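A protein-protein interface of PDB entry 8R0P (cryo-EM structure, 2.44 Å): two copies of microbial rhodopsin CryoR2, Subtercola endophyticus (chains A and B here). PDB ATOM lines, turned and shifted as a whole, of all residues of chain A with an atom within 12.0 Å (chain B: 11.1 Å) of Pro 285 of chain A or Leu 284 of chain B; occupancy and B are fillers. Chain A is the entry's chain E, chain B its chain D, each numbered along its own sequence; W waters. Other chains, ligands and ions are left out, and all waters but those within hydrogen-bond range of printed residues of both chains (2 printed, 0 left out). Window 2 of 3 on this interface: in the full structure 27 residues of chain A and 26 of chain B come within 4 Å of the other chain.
Water W1 bridges OD1 of Asp 266 of chain A and N of Ser 271 of chain B.
Water W2 lies within hydrogen-bond range of the side-chain carboxylate (OD1) of Asp 266 of chain A (2.6 Å), the side-chain amino group (NZ) of Lys 278 of chain B (3.1 Å) and the backbone NH (N) of Ala 282 of chain B (3.3 Å).
The backbone carbonyl oxygen (O) of Asp 265 of chain A sits at hydrogen-bond distance from the side-chain amino group (NZ) of Lys 278 of chain B (3.1 Å).
The backbone carbonyl oxygen (O) of Ser 271 of chain B is in hydrogen-bond range of the side-chain hydroxyl (OG) of Ser 49 of chain A (3.0 Å).
OG of Ser 271 of chain B is in hydrogen-bond range of OD2 of Asp 266 of chain A (2.7 Å).
Of the printed residues of chain B, Ser 49 of chain A touches Glu 270 and Ser 271.
Printed residues of chain B within 4 Å of Asp 265 of chain A: Lys 278.
Printed residues of chain B within 4 Å of Asp 266 of chain A: Ser 271.
No residue of chain B comes within 4 Å of Gly 283 of chain A.
No residue of chain B comes within 4 Å of Leu 284 of chain A.
Pro 285 of chain A touches three residues of chain B.
Gly 264 of chain B touches none of the printed residues of chain A.
No residue of chain A comes within 4 Å of Val 267 of chain B.
No residue of chain A comes within 4 Å of Pro 269 of chain B.
Of the printed residues of chain A, Ser 271 of chain B touches Ser 49 (3.0 Å) and Asp 266 (2.7 Å).
Of the printed residues of chain A, Lys 278 of chain B touches Asp 265.
Asp 281 of chain B touches none of the printed residues of chain A.
Ala 282 of chain B touches one residue of chain A.
Of chain A, only Pro 285 comes within 4 Å of Gly 283 of chain B.
Of the printed residues of chain A, Leu 284 of chain B touches Pro 285 (3.7 Å).
Pro 285 of chain B touches none of the printed residues of chain A.
No residue of chain A comes within 4 Å of Arg 286 of chain B.
The nearest residue of chain B that does not touch Pro 285 of chain A is Pro 269 of chain B (4.2 Å).
The nearest printed residue of chain A that does not touch Ser 271 of chain B is Asp 265 of chain A (5.9 Å).
Of the 16 printed residues of chain A, 4 touch a printed residue of chain B.
Hydrophobic or aromatic side chains of chain A within 4 Å of the printed part of chain B: Pro 285.
Of the 18 printed residues of chain B, 6 touch a printed residue of chain A.
Hydrophobic or aromatic side chains of chain B within 4 Å of the printed part of chain A: Ala 282 and Leu 284.
Along chain B the printed residues that touch a printed residue of chain A span positions 270 to 284.
Among the printed residues, 7 pairs touch across the chains.
Ser 49 of chain A touches Glu 270 of chain B (CB to OE2, 3.5 Å).
Pro 285 of chain A touches Ala 282 of chain B (CB to C, 3.7 Å).
Pro 285 of chain A touches Gly 283 of chain B (CB to N, 3.5 Å).
O of Pro 285 of chain A touches CD1 of Leu 284 of chain B, 3.7 Å away.
ND1 of His 268 of chain B is in hydrogen-bond range of O of Glu 270 of chain B, 3.1 Å away.
The backbone NH of Asp 265 of chain A lies within hydrogen-bond range of the backbone carbonyl oxygen of Asp 260 of chain A, 3.0 Å away.
The backbone NH (N) of Gly 283 of chain B is in hydrogen-bond range of the backbone carbonyl oxygen (O) of His 268 of chain B.
The side-chain amino group of Lys 278 of chain B lies within salt-bridge range of the side-chain carboxylate of Asp 281 of chain B (3.1 Å).
The backbone carbonyl oxygen (O) of Asp 260 of chain A sits at hydrogen-bond distance from the backbone NH (N) of Asp 266 of chain A, 3.4 Å away.
Pro 285 of chain A touches Ala 282 of chain B, but with the chains exchanged Ala 282 of chain A does not touch Pro 285 of chain B (15.5 Å).
Pro 285 of chain A touches Gly 283 of chain B, but with the chains exchanged Gly 283 of chain A does not touch Pro 285 of chain B (11.8 Å).
Pro 285 of chain A touches Leu 284 of chain B, but with the chains exchanged Leu 284 of chain A does not touch Pro 285 of chain B (8.7 Å).
Of the 7 pairs that touch across the chains among the printed residues, none has its exchanged pair printed and touching as well.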
ATOM      1  N   SER A  49      -2.622   4.363 -12.755  1.00  0.00           N
ATOM      2  CA  SER A  49      -3.200   5.570 -13.320  1.00  0.00           C
ATOM      3  C   SER A  49      -4.307   5.246 -14.326  1.00  0.00           C
ATOM      4  O   SER A  49      -5.282   5.985 -14.422  1.00  0.00           O
ATOM      5  CB  SER A  49      -2.110   6.417 -13.944  1.00  0.00           C
ATOM      6  OG  SER A  49      -1.534   5.789 -15.086  1.00  0.00           O
ATOM      7  N   ASP A 260      -1.515  -5.634 -16.479  1.00  0.00           N
ATOM      8  CA  ASP A 260      -0.779  -4.746 -17.358  1.00  0.00           C
ATOM      9  C   ASP A 260       0.704  -4.828 -17.048  1.00  0.00           C
ATOM     10  O   ASP A 260       1.528  -5.055 -17.923  1.00  0.00           O
ATOM     11  CB  ASP A 260      -1.222  -3.312 -17.163  1.00  0.00           C
ATOM     12  CG  ASP A 260      -2.665  -3.037 -17.578  1.00  0.00           C
ATOM     13  OD1 ASP A 260      -3.377  -4.003 -17.974  1.00  0.00           O
ATOM     14  OD2 ASP A 260      -3.081  -1.845 -17.487  1.00  0.00           O
ATOM     15  N   VAL A 261       1.020  -4.771 -15.757  1.00  0.00           N
ATOM     16  CA  VAL A 261       2.378  -4.966 -15.309  1.00  0.00           C
ATOM     17  C   VAL A 261       2.921  -6.317 -15.723  1.00  0.00           C
ATOM     18  O   VAL A 261       4.091  -6.409 -16.061  1.00  0.00           O
ATOM     19  CB  VAL A 261       2.500  -4.794 -13.817  1.00  0.00           C
ATOM     20  CG1 VAL A 261       3.861  -5.245 -13.410  1.00  0.00           C
ATOM     21  CG2 VAL A 261       2.256  -3.379 -13.360  1.00  0.00           C
ATOM     22  N   GLY A 264       3.849  -6.236 -19.436  1.00  0.00           N
ATOM     23  CA  GLY A 264       4.870  -5.278 -19.826  1.00  0.00           C
ATOM     24  C   GLY A 264       4.252  -4.031 -20.455  1.00  0.00           C
ATOM     25  O   GLY A 264       4.927  -3.246 -21.106  1.00  0.00           O
ATOM     26  N   ASP A 265       2.950  -3.878 -20.289  1.00  0.00           N
ATOM     27  CA  ASP A 265       2.248  -2.707 -20.749  1.00  0.00           C
ATOM     28  C   ASP A 265       2.409  -1.566 -19.751  1.00  0.00           C
ATOM     29  O   ASP A 265       2.182  -0.411 -20.080  1.00  0.00           O
ATOM     30  CB  ASP A 265       0.778  -3.062 -20.923  1.00  0.00           C
ATOM     31  CG  ASP A 265       0.601  -4.157 -21.959  1.00  0.00           C
ATOM     32  OD1 ASP A 265       1.634  -4.557 -22.579  1.00  0.00           O
ATOM     33  OD2 ASP A 265      -0.560  -4.610 -22.140  1.00  0.00           O
ATOM     34  N   ASP A 266       2.690  -1.877 -18.494  1.00  0.00           N
ATOM     35  CA  ASP A 266       2.943  -0.807 -17.569  1.00  0.00           C
ATOM     36  C   ASP A 266       3.908  -1.286 -16.497  1.00  0.00           C
ATOM     37  O   ASP A 266       4.450  -2.374 -16.583  1.00  0.00           O
ATOM     38  CB  ASP A 266       1.652  -0.229 -17.005  1.00  0.00           C
ATOM     39  CG  ASP A 266       1.647   1.307 -16.976  1.00  0.00           C
ATOM     40  OD1 ASP A 266       2.688   1.934 -16.554  1.00  0.00           O
ATOM     41  OD2 ASP A 266       0.610   1.900 -17.408  1.00  0.00           O
ATOM     42  N   VAL A 267       4.178  -0.394 -15.569  1.00  0.00           N
ATOM     43  CA  VAL A 267       5.005  -0.683 -14.433  1.00  0.00           C
ATOM     44  C   VAL A 267       4.243  -0.130 -13.248  1.00  0.00           C
ATOM     45  O   VAL A 267       3.340   0.657 -13.415  1.00  0.00           O
ATOM     46  CB  VAL A 267       6.431  -0.088 -14.562  1.00  0.00           C
ATOM     47  CG1 VAL A 267       7.132  -0.626 -15.774  1.00  0.00           C
ATOM     48  CG2 VAL A 267       6.480   1.419 -14.679  1.00  0.00           C
ATOM     49  N   HIS A 268       4.597  -0.585 -12.064  1.00  0.00           N
ATOM     50  CA  HIS A 268       3.935  -0.132 -10.871  1.00  0.00           C
ATOM     51  C   HIS A 268       5.007  -0.132  -9.806  1.00  0.00           C
ATOM     52  O   HIS A 268       5.820  -1.045  -9.681  1.00  0.00           O
ATOM     53  CB  HIS A 268       2.742  -1.040 -10.553  1.00  0.00           C
ATOM     54  CG  HIS A 268       1.806  -0.431  -9.594  1.00  0.00           C
ATOM     55  ND1 HIS A 268       1.765  -0.784  -8.257  1.00  0.00           N
ATOM     56  CD2 HIS A 268       0.928   0.585  -9.769  1.00  0.00           C
ATOM     57  CE1 HIS A 268       0.845  -0.011  -7.656  1.00  0.00           C
ATOM     58  NE2 HIS A 268       0.315   0.828  -8.558  1.00  0.00           N
ATOM     59  N   PRO A 269       5.066   0.921  -9.012  1.00  0.00           N
ATOM     60  CA  PRO A 269       6.139   1.095  -8.056  1.00  0.00           C
ATOM     61  C   PRO A 269       6.229   0.088  -6.919  1.00  0.00           C
ATOM     62  O   PRO A 269       7.252   0.046  -6.239  1.00  0.00           O
ATOM     63  CB  PRO A 269       5.706   2.387  -7.391  1.00  0.00           C
ATOM     64  CG  PRO A 269       4.981   3.070  -8.470  1.00  0.00           C
ATOM     65  CD  PRO A 269       4.087   1.987  -8.983  1.00  0.00           C
ATOM     66  N   GLU A 270       5.116  -0.587  -6.616  1.00  0.00           N
ATOM     67  CA  GLU A 270       5.064  -1.492  -5.485  1.00  0.00           C
ATOM     68  C   GLU A 270       4.489  -2.799  -5.979  1.00  0.00           C
ATOM     69  O   GLU A 270       3.791  -2.801  -6.995  1.00  0.00           O
ATOM     70  CB  GLU A 270       4.243  -0.897  -4.348  1.00  0.00           C
ATOM     71  CG  GLU A 270       2.833  -0.561  -4.756  1.00  0.00           C
ATOM     72  CD  GLU A 270       1.807  -0.426  -3.627  1.00  0.00           C
ATOM     73  OE1 GLU A 270       2.068   0.411  -2.716  1.00  0.00           O
ATOM     74  OE2 GLU A 270       0.716  -1.126  -3.681  1.00  0.00           O
ATOM     75  N   ASP A 281       5.025  -7.797  -9.413  1.00  0.00           N
ATOM     76  CA  ASP A 281       6.172  -7.249  -8.687  1.00  0.00           C
ATOM     77  C   ASP A 281       6.327  -5.754  -8.923  1.00  0.00           C
ATOM     78  O   ASP A 281       5.861  -5.238  -9.925  1.00  0.00           O
ATOM     79  CB  ASP A 281       7.464  -7.873  -9.145  1.00  0.00           C
ATOM     80  CG  ASP A 281       7.459  -9.381  -9.084  1.00  0.00           C
ATOM     81  OD1 ASP A 281       6.442  -9.953  -8.592  1.00  0.00           O
ATOM     82  OD2 ASP A 281       8.459  -9.988  -9.561  1.00  0.00           O
ATOM     83  N   ALA A 282       6.984  -5.055  -7.994  1.00  0.00           N
ATOM     84  CA  ALA A 282       7.352  -3.656  -8.204  1.00  0.00           C
ATOM     85  C   ALA A 282       8.326  -3.559  -9.381  1.00  0.00           C
ATOM     86  O   ALA A 282       9.018  -4.519  -9.755  1.00  0.00           O
ATOM     87  CB  ALA A 282       7.941  -3.029  -6.963  1.00  0.00           C
ATOM     88  N   GLY A 283       8.365  -2.379  -9.985  1.00  0.00           N
ATOM     89  CA  GLY A 283       9.195  -2.198 -11.162  1.00  0.00           C
ATOM     90  C   GLY A 283       9.400  -0.725 -11.387  1.00  0.00           C
ATOM     91  O   GLY A 283       8.637   0.052 -10.852  1.00  0.00           O
ATOM     92  N   LEU A 284      10.464  -0.363 -12.111  1.00  0.00           N
ATOM     93  CA  LEU A 284      10.710   1.034 -12.438  1.00  0.00           C
ATOM     94  C   LEU A 284      10.533   1.234 -13.922  1.00  0.00           C
ATOM     95  O   LEU A 284      10.755   0.322 -14.713  1.00  0.00           O
ATOM     96  CB  LEU A 284      12.121   1.436 -12.024  1.00  0.00           C
ATOM     97  CG  LEU A 284      12.275   1.603 -10.523  1.00  0.00           C
ATOM     98  CD1 LEU A 284      13.727   1.786 -10.149  1.00  0.00           C
ATOM     99  CD2 LEU A 284      11.429   2.760 -10.059  1.00  0.00           C
ATOM    100  N   PRO A 285      10.156   2.468 -14.312  1.00  0.00           N
ATOM    101  CA  PRO A 285       9.976   2.842 -15.708  1.00  0.00           C
ATOM    102  C   PRO A 285      11.305   2.542 -16.330  1.00  0.00           C
ATOM    103  O   PRO A 285      12.307   3.030 -15.833  1.00  0.00           O
ATOM    104  CB  PRO A 285       9.751   4.325 -15.653  1.00  0.00           C
ATOM    105  CG  PRO A 285       9.204   4.556 -14.293  1.00  0.00           C
ATOM    106  CD  PRO A 285       9.942   3.585 -13.400  1.00  0.00           C
ATOM    107  N   ARG A 286      11.336   1.692 -17.344  1.00  0.00           N
ATOM    108  CA  ARG A 286      12.594   1.401 -18.023  1.00  0.00           C
ATOM    109  C   ARG A 286      12.611   2.039 -19.421  1.00  0.00           C
ATOM    110  O   ARG A 286      13.728   2.137 -19.987  1.00  0.00           O
ATOM    111  CB  ARG A 286      12.852  -0.110 -18.124  1.00  0.00           C
ATOM    112  N   VAL B 261       6.349  14.631 -22.872  1.00  0.00           N
ATOM    113  CA  VAL B 261       6.934  13.328 -22.667  1.00  0.00           C
ATOM    114  C   VAL B 261       7.175  12.605 -23.975  1.00  0.00           C
ATOM    115  O   VAL B 261       8.177  11.920 -24.101  1.00  0.00           O
ATOM    116  CB  VAL B 261       6.092  12.479 -21.752  1.00  0.00           C
ATOM    117  CG1 VAL B 261       6.632  11.090 -21.785  1.00  0.00           C
ATOM    118  CG2 VAL B 261       6.051  12.993 -20.335  1.00  0.00           C
ATOM    119  N   GLY B 264      10.276  14.055 -25.687  1.00  0.00           N
ATOM    120  CA  GLY B 264      11.528  13.946 -24.956  1.00  0.00           C
ATOM    121  C   GLY B 264      11.891  15.264 -24.276  1.00  0.00           C
ATOM    122  O   GLY B 264      13.021  15.476 -23.862  1.00  0.00           O
ATOM    123  N   ASP B 265      10.926  16.165 -24.198  1.00  0.00           N
ATOM    124  CA  ASP B 265      11.096  17.415 -23.502  1.00  0.00           C
ATOM    125  C   ASP B 265      10.899  17.220 -22.004  1.00  0.00           C
ATOM    126  O   ASP B 265      11.314  18.050 -21.206  1.00  0.00           O
ATOM    127  CB  ASP B 265      10.086  18.414 -24.049  1.00  0.00           C
ATOM    128  CG  ASP B 265      10.312  18.661 -25.530  1.00  0.00           C
ATOM    129  OD1 ASP B 265      11.312  18.101 -26.077  1.00  0.00           O
ATOM    130  OD2 ASP B 265       9.489  19.401 -26.133  1.00  0.00           O
ATOM    131  N   ASP B 266      10.173  16.187 -21.604  1.00  0.00           N
ATOM    132  CA  ASP B 266      10.071  15.934 -20.194  1.00  0.00           C
ATOM    133  C   ASP B 266       9.887  14.443 -19.962  1.00  0.00           C
ATOM    134  O   ASP B 266       9.988  13.649 -20.877  1.00  0.00           O
ATOM    135  CB  ASP B 266       8.995  16.788 -19.536  1.00  0.00           C
ATOM    136  CG  ASP B 266       9.460  17.408 -18.207  1.00  0.00           C
ATOM    137  OD1 ASP B 266      10.107  16.679 -17.357  1.00  0.00           O
ATOM    138  OD2 ASP B 266       9.209  18.636 -18.015  1.00  0.00           O
ATOM    139  N   VAL B 267       9.735  14.102 -18.701  1.00  0.00           N
ATOM    140  CA  VAL B 267       9.473  12.755 -18.283  1.00  0.00           C
ATOM    141  C   VAL B 267       8.338  12.876 -17.288  1.00  0.00           C
ATOM    142  O   VAL B 267       8.065  13.945 -16.794  1.00  0.00           O
ATOM    143  CB  VAL B 267      10.723  12.059 -17.686  1.00  0.00           C
ATOM    144  CG1 VAL B 267      11.834  12.000 -18.692  1.00  0.00           C
ATOM    145  CG2 VAL B 267      11.295  12.728 -16.455  1.00  0.00           C
ATOM    146  N   HIS B 268       7.667  11.769 -17.042  1.00  0.00           N
ATOM    147  CA  HIS B 268       6.563  11.764 -16.121  1.00  0.00           C
ATOM    148  C   HIS B 268       6.609  10.403 -15.469  1.00  0.00           C
ATOM    149  O   HIS B 268       6.816   9.367 -16.101  1.00  0.00           O
ATOM    150  CB  HIS B 268       5.255  12.057 -16.862  1.00  0.00           C
ATOM    151  CG  HIS B 268       4.163  12.442 -15.954  1.00  0.00           C
ATOM    152  ND1 HIS B 268       3.151  11.573 -15.587  1.00  0.00           N
ATOM    153  CD2 HIS B 268       3.973  13.591 -15.265  1.00  0.00           C
ATOM    154  CE1 HIS B 268       2.350  12.212 -14.717  1.00  0.00           C
ATOM    155  NE2 HIS B 268       2.827  13.449 -14.511  1.00  0.00           N
ATOM    156  N   PRO B 269       6.448  10.359 -14.158  1.00  0.00           N
ATOM    157  CA  PRO B 269       6.622   9.134 -13.410  1.00  0.00           C
ATOM    158  C   PRO B 269       5.644   8.003 -13.691  1.00  0.00           C
ATOM    159  O   PRO B 269       5.893   6.876 -13.270  1.00  0.00           O
ATOM    160  CB  PRO B 269       6.267   9.612 -12.015  1.00  0.00           C
ATOM    161  CG  PRO B 269       6.676  11.020 -12.053  1.00  0.00           C
ATOM    162  CD  PRO B 269       6.072  11.489 -13.336  1.00  0.00           C
ATOM    163  N   GLU B 270       4.468   8.345 -14.234  1.00  0.00           N
ATOM    164  CA  GLU B 270       3.404   7.382 -14.426  1.00  0.00           C
ATOM    165  C   GLU B 270       2.943   7.507 -15.862  1.00  0.00           C
ATOM    166  O   GLU B 270       3.125   8.570 -16.461  1.00  0.00           O
ATOM    167  CB  GLU B 270       2.317   7.641 -13.389  1.00  0.00           C
ATOM    168  CG  GLU B 270       1.109   8.305 -13.901  1.00  0.00           C
ATOM    169  CD  GLU B 270       0.185   9.095 -12.997  1.00  0.00           C
ATOM    170  OE1 GLU B 270       0.306   9.113 -11.735  1.00  0.00           O
ATOM    171  OE2 GLU B 270      -0.723   9.630 -13.651  1.00  0.00           O
ATOM    172  N   SER B 271       2.299   6.470 -16.389  1.00  0.00           N
ATOM    173  CA  SER B 271       1.713   6.616 -17.712  1.00  0.00           C
ATOM    174  C   SER B 271       0.527   7.576 -17.648  1.00  0.00           C
ATOM    175  O   SER B 271      -0.017   7.836 -16.582  1.00  0.00           O
ATOM    176  CB  SER B 271       1.337   5.333 -18.317  1.00  0.00           C
ATOM    177  OG  SER B 271       0.534   4.616 -17.420  1.00  0.00           O
ATOM    178  N   ILE B 272       0.185   8.162 -18.788  1.00  0.00           N
ATOM    179  CA  ILE B 272      -0.927   9.092 -18.831  1.00  0.00           C
ATOM    180  C   ILE B 272      -1.992   8.497 -19.716  1.00  0.00           C
ATOM    181  O   ILE B 272      -1.696   7.997 -20.796  1.00  0.00           O
ATOM    182  CB  ILE B 272      -0.479  10.492 -19.304  1.00  0.00           C
ATOM    183  CG1 ILE B 272       0.464  11.129 -18.279  1.00  0.00           C
ATOM    184  CG2 ILE B 272      -1.696  11.369 -19.559  1.00  0.00           C
ATOM    185  CD1 ILE B 272       1.111  12.390 -18.726  1.00  0.00           C
ATOM    186  N   LYS B 278      -3.804   5.278 -23.917  1.00  0.00           N
ATOM    187  CA  LYS B 278      -2.525   5.656 -23.331  1.00  0.00           C
ATOM    188  C   LYS B 278      -1.928   6.767 -24.175  1.00  0.00           C
ATOM    189  O   LYS B 278      -1.823   6.637 -25.393  1.00  0.00           O
ATOM    190  CB  LYS B 278      -1.530   4.495 -23.303  1.00  0.00           C
ATOM    191  CG  LYS B 278      -0.355   4.652 -22.360  1.00  0.00           C
ATOM    192  CD  LYS B 278       0.573   3.467 -22.445  1.00  0.00           C
ATOM    193  CE  LYS B 278       1.411   3.311 -21.195  1.00  0.00           C
ATOM    194  NZ  LYS B 278       2.506   2.332 -21.390  1.00  0.00           N
ATOM    195  N   SER B 280       1.063   8.705 -22.911  1.00  0.00           N
ATOM    196  CA  SER B 280       2.502   8.637 -22.711  1.00  0.00           C
ATOM    197  C   SER B 280       2.823   7.494 -21.751  1.00  0.00           C
ATOM    198  O   SER B 280       2.019   7.216 -20.870  1.00  0.00           O
ATOM    199  CB  SER B 280       3.035   9.975 -22.166  1.00  0.00           C
ATOM    200  OG  SER B 280       2.547  10.242 -20.834  1.00  0.00           O
ATOM    201  N   ASP B 281       4.048   6.946 -21.822  1.00  0.00           N
ATOM    202  CA  ASP B 281       4.532   5.952 -20.863  1.00  0.00           C
ATOM    203  C   ASP B 281       5.243   6.601 -19.686  1.00  0.00           C
ATOM    204  O   ASP B 281       5.735   7.712 -19.800  1.00  0.00           O
ATOM    205  CB  ASP B 281       5.538   5.023 -21.493  1.00  0.00           C
ATOM    206  CG  ASP B 281       5.038   4.359 -22.752  1.00  0.00           C
ATOM    207  OD1 ASP B 281       3.840   4.570 -23.099  1.00  0.00           O
ATOM    208  OD2 ASP B 281       5.858   3.657 -23.408  1.00  0.00           O
ATOM    209  N   ALA B 282       5.300   5.901 -18.549  1.00  0.00           N
ATOM    210  CA  ALA B 282       6.116   6.343 -17.420  1.00  0.00           C
ATOM    211  C   ALA B 282       7.592   6.349 -17.828  1.00  0.00           C
ATOM    212  O   ALA B 282       8.025   5.662 -18.767  1.00  0.00           O
ATOM    213  CB  ALA B 282       5.899   5.493 -16.193  1.00  0.00           C
ATOM    214  N   GLY B 283       8.371   7.155 -17.121  1.00  0.00           N
ATOM    215  CA  GLY B 283       9.773   7.296 -17.474  1.00  0.00           C
ATOM    216  C   GLY B 283      10.508   7.901 -16.309  1.00  0.00           C
ATOM    217  O   GLY B 283       9.864   8.478 -15.457  1.00  0.00           O
ATOM    218  N   LEU B 284      11.828   7.699 -16.251  1.00  0.00           N
ATOM    219  CA  LEU B 284      12.638   8.301 -15.201  1.00  0.00           C
ATOM    220  C   LEU B 284      13.551   9.333 -15.811  1.00  0.00           C
ATOM    221  O   LEU B 284      13.946   9.222 -16.970  1.00  0.00           O
ATOM    222  CB  LEU B 284      13.459   7.230 -14.493  1.00  0.00           C
ATOM    223  CG  LEU B 284      12.629   6.360 -13.566  1.00  0.00           C
ATOM    224  CD1 LEU B 284      13.435   5.184 -13.063  1.00  0.00           C
ATOM    225  CD2 LEU B 284      12.099   7.203 -12.434  1.00  0.00           C
ATOM    226  N   PRO B 285      13.931  10.342 -15.002  1.00  0.00           N
ATOM    227  CA  PRO B 285      14.838  11.399 -15.419  1.00  0.00           C
ATOM    228  C   PRO B 285      16.071  10.662 -15.850  1.00  0.00           C
ATOM    229  O   PRO B 285      16.584   9.870 -15.074  1.00  0.00           O
ATOM    230  CB  PRO B 285      15.110  12.156 -14.152  1.00  0.00           C
ATOM    231  CG  PRO B 285      13.917  11.894 -13.309  1.00  0.00           C
ATOM    232  CD  PRO B 285      13.531  10.464 -13.606  1.00  0.00           C
ATOM    233  N   ARG B 286      16.497  10.843 -17.088  1.00  0.00           N
ATOM    234  CA  ARG B 286      17.720  10.195 -17.551  1.00  0.00           C
ATOM    235  C   ARG B 286      18.847  11.226 -17.713  1.00  0.00           C
ATOM    236  O   ARG B 286      20.018  10.777 -17.796  1.00  0.00           O
ATOM    237  CB  ARG B 286      17.494   9.445 -18.872  1.00  0.00           C
HETATM  238  O   HOH W   1       2.511   3.780 -14.906  1.00  0.00           O
HETATM  239  O   HOH W   2       3.945   2.928 -18.653  1.00  0.00           O
